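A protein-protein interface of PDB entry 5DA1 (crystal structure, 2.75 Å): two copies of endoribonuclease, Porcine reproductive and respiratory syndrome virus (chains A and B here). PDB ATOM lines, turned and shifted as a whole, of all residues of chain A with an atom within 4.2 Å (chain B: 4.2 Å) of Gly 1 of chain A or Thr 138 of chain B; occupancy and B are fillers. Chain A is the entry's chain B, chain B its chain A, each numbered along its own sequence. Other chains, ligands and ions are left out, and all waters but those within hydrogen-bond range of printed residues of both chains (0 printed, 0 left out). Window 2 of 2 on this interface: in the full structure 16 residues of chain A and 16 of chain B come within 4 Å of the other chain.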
ATOM      1  N   GLY A   1     -12.346  14.209   0.883  1.00  0.00           N
ATOM      2  CA  GLY A   1     -13.814  14.129   0.540  1.00  0.00           C
ATOM      3  C   GLY A   1     -14.466  15.487   0.363  1.00  0.00           C
ATOM      4  O   GLY A   1     -13.938  16.472   0.825  1.00  0.00           O
ATOM      5  N   SER A   2     -15.598  15.568  -0.322  1.00  0.00           N
ATOM      6  CA  SER A   2     -16.267  16.854  -0.473  1.00  0.00           C
ATOM      7  C   SER A   2     -17.723  16.793  -0.051  1.00  0.00           C
ATOM      8  O   SER A   2     -18.368  15.747  -0.169  1.00  0.00           O
ATOM      9  CB  SER A   2     -16.204  17.337  -1.929  1.00  0.00           C
ATOM     10  OG  SER A   2     -17.100  18.433  -2.146  1.00  0.00           O
ATOM     11  N   LEU A  54     -14.530  21.084  -2.300  1.00  0.00           N
ATOM     12  CA  LEU A  54     -14.352  21.944  -1.142  1.00  0.00           C
ATOM     13  C   LEU A  54     -13.244  22.978  -1.338  1.00  0.00           C
ATOM     14  O   LEU A  54     -13.052  23.870  -0.512  1.00  0.00           O
ATOM     15  CB  LEU A  54     -14.141  21.109   0.120  1.00  0.00           C
ATOM     16  CG  LEU A  54     -15.455  20.697   0.800  1.00  0.00           C
ATOM     17  CD1 LEU A  54     -15.204  19.644   1.846  1.00  0.00           C
ATOM     18  CD2 LEU A  54     -16.176  21.878   1.421  1.00  0.00           C
ATOM     19  N   ARG A  55     -12.534  22.854  -2.454  1.00  0.00           N
ATOM     20  CA  ARG A  55     -11.562  23.847  -2.907  1.00  0.00           C
ATOM     21  C   ARG A  55     -11.865  24.177  -4.360  1.00  0.00           C
ATOM     22  O   ARG A  55     -12.350  23.300  -5.090  1.00  0.00           O
ATOM     23  CB  ARG A  55     -10.135  23.337  -2.705  1.00  0.00           C
ATOM     24  CG  ARG A  55      -9.668  23.663  -1.308  1.00  0.00           C
ATOM     25  CD  ARG A  55      -8.565  22.771  -0.802  1.00  0.00           C
ATOM     26  NE  ARG A  55      -8.560  22.813   0.666  1.00  0.00           N
ATOM     27  CZ  ARG A  55      -7.517  22.545   1.465  1.00  0.00           C
ATOM     28  NH1 ARG A  55      -6.328  22.197   0.972  1.00  0.00           N
ATOM     29  NH2 ARG A  55      -7.675  22.628   2.786  1.00  0.00           N
ATOM     30  N   LYS B 136      -7.318  17.001   7.940  1.00  0.00           N
ATOM     31  CA  LYS B 136      -6.089  17.245   7.190  1.00  0.00           C
ATOM     32  C   LYS B 136      -6.460  17.697   5.795  1.00  0.00           C
ATOM     33  O   LYS B 136      -6.843  16.897   4.936  1.00  0.00           O
ATOM     34  CB  LYS B 136      -5.131  16.033   7.179  1.00  0.00           C
ATOM     35  CG  LYS B 136      -3.834  16.309   7.959  1.00  0.00           C
ATOM     36  CD  LYS B 136      -3.565  15.204   8.963  1.00  0.00           C
ATOM     37  CE  LYS B 136      -3.388  15.790  10.367  1.00  0.00           C
ATOM     38  NZ  LYS B 136      -3.347  14.700  11.399  1.00  0.00           N
ATOM     39  N   GLY B 137      -6.359  19.007   5.604  1.00  0.00           N
ATOM     40  CA  GLY B 137      -6.797  19.637   4.381  1.00  0.00           C
ATOM     41  C   GLY B 137      -8.276  19.382   4.194  1.00  0.00           C
ATOM     42  O   GLY B 137      -9.102  19.970   4.867  1.00  0.00           O
ATOM     43  N   THR B 138      -8.574  18.458   3.298  1.00  0.00           N
ATOM     44  CA  THR B 138      -9.906  18.201   2.793  1.00  0.00           C
ATOM     45  C   THR B 138     -10.579  17.013   3.513  1.00  0.00           C
ATOM     46  O   THR B 138     -11.757  16.728   3.281  1.00  0.00           O
ATOM     47  CB  THR B 138      -9.822  18.055   1.225  1.00  0.00           C
ATOM     48  OG1 THR B 138     -10.440  19.189   0.623  1.00  0.00           O
ATOM     49  CG2 THR B 138     -10.436  16.771   0.647  1.00  0.00           C
ATOM     50  N   THR B 139      -9.850  16.367   4.424  1.00  0.00           N
ATOM     51  CA  THR B 139     -10.331  15.163   5.083  1.00  0.00           C
ATOM     52  C   THR B 139     -10.445  15.300   6.593  1.00  0.00           C
ATOM     53  O   THR B 139      -9.489  15.712   7.252  1.00  0.00           O
ATOM     54  CB  THR B 139      -9.380  13.984   4.830  1.00  0.00           C
ATOM     55  OG1 THR B 139      -8.667  14.196   3.602  1.00  0.00           O
ATOM     56  CG2 THR B 139     -10.182  12.650   4.781  1.00  0.00           C
ATOM     57  N   LYS B 170     -14.322  23.373   5.350  1.00  0.00           N
ATOM     58  CA  LYS B 170     -12.938  22.849   5.410  1.00  0.00           C
ATOM     59  C   LYS B 170     -12.779  21.417   4.904  1.00  0.00           C
ATOM     60  O   LYS B 170     -11.977  21.149   4.015  1.00  0.00           O
ATOM     61  CB  LYS B 170     -12.417  22.885   6.856  1.00  0.00           C
ATOM     62  CG  LYS B 170     -12.468  24.246   7.527  1.00  0.00           C
ATOM     63  CD  LYS B 170     -11.075  24.881   7.576  1.00  0.00           C
ATOM     64  CE  LYS B 170     -11.167  26.411   7.629  1.00  0.00           C
ATOM     65  NZ  LYS B 170     -12.173  26.795   8.665  1.00  0.00           N
ATOM     66  N   ALA B 171     -13.527  20.500   5.512  1.00  0.00           N
ATOM     67  CA  ALA B 171     -13.436  19.081   5.191  1.00  0.00           C
ATOM     68  C   ALA B 171     -14.804  18.342   5.176  1.00  0.00           C
ATOM     69  O   ALA B 171     -15.819  18.878   5.673  1.00  0.00           O
ATOM     70  CB  ALA B 171     -12.470  18.434   6.146  1.00  0.00           C
ATOM     71  N   ALA B 172     -14.824  17.130   4.605  1.00  0.00           N
ATOM     72  CA  ALA B 172     -16.010  16.254   4.610  1.00  0.00           C
ATOM     73  C   ALA B 172     -15.631  14.774   4.436  1.00  0.00           C
ATOM     74  O   ALA B 172     -14.620  14.483   3.765  1.00  0.00           O
ATOM     75  CB  ALA B 172     -16.946  16.652   3.502  1.00  0.00           C
ATOM     76  N   LYS B 173     -16.412  13.842   5.014  1.00  0.00           N
ATOM     77  CA  LYS B 173     -16.250  12.387   4.755  1.00  0.00           C
ATOM     78  C   LYS B 173     -17.560  11.723   4.533  1.00  0.00           C
ATOM     79  O   LYS B 173     -18.467  11.830   5.372  1.00  0.00           O
ATOM     80  CB  LYS B 173     -15.626  11.637   5.939  1.00  0.00           C
ATOM     81  CG  LYS B 173     -14.100  11.584   5.989  1.00  0.00           C
ATOM     82  CD  LYS B 173     -13.483  12.992   5.755  1.00  0.00           C
ATOM     83  CE  LYS B 173     -14.218  14.075   6.624  1.00  0.00           C
ATOM     84  NZ  LYS B 173     -14.110  15.499   6.152  1.00  0.00           N
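The backbone carbonyl oxygen of Gly 1 of chain A sits close to the backbone carbonyl oxygen of Thr 138 of chain B, 3.3 Å away.
Among the printed residues, pairs that only touch across the chains: Gly 1 of chain A with Ala 172 of chain B (3.3 Å), Ser 2 of chain A with Ala 172 of chain B (3.6 Å), Leu 54 of chain A with Ala 171 of chain B (3.6 Å), Leu 54 of chain A with Ala 172 of chain B (3.8 Å) and Arg 55 of chain A with Gly 137 of chain B (3.5 Å).
No position is printed for both chains.
The backbone NH (N) of Ala 172 of chain B lies within hydrogen-bond range of the backbone carbonyl oxygen (O) of Thr 138 of chain B (3.4 Å).
Of the 4 printed residues of chain A, 4 touch a printed residue of chain B. Of the 8 printed residues of chain B, 4 touch a printed residue of chain A. Hydrophobic or aromatic side chains of chain B within 4 Å of the printed part of chain A: Ala 172.
Of chain B, only Thr 138 (3.2 Å) and Ala 172 (3.3 Å) come within 4 Å of Gly 1 of chain A. Of the printed residues of chain B, Leu 54 of chain A touches Ala 171 and Ala 172. Printed residues of chain B within 4 Å of Arg 55 of chain A: Gly 137 (3.5 Å). Printed residues of chain A within 4 Å of Gly 137 of chain B: Arg 55 (3.5 Å). Thr 138 of chain B touches one residue of chain A. Thr 139 of chain B touches none of the printed residues of chain A. Of the printed residues of chain A, Ala 171 of chain B touches Leu 54. Printed residues of chain A within 4 Å of Ala 172 of chain B: Gly 1 (3.3 Å), Ser 2 (3.6 Å) and Leu 54 (3.8 Å). The nearest printed residue of chain B that does not touch Leu 54 of chain A is Lys 170 of chain B (4.2 Å).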
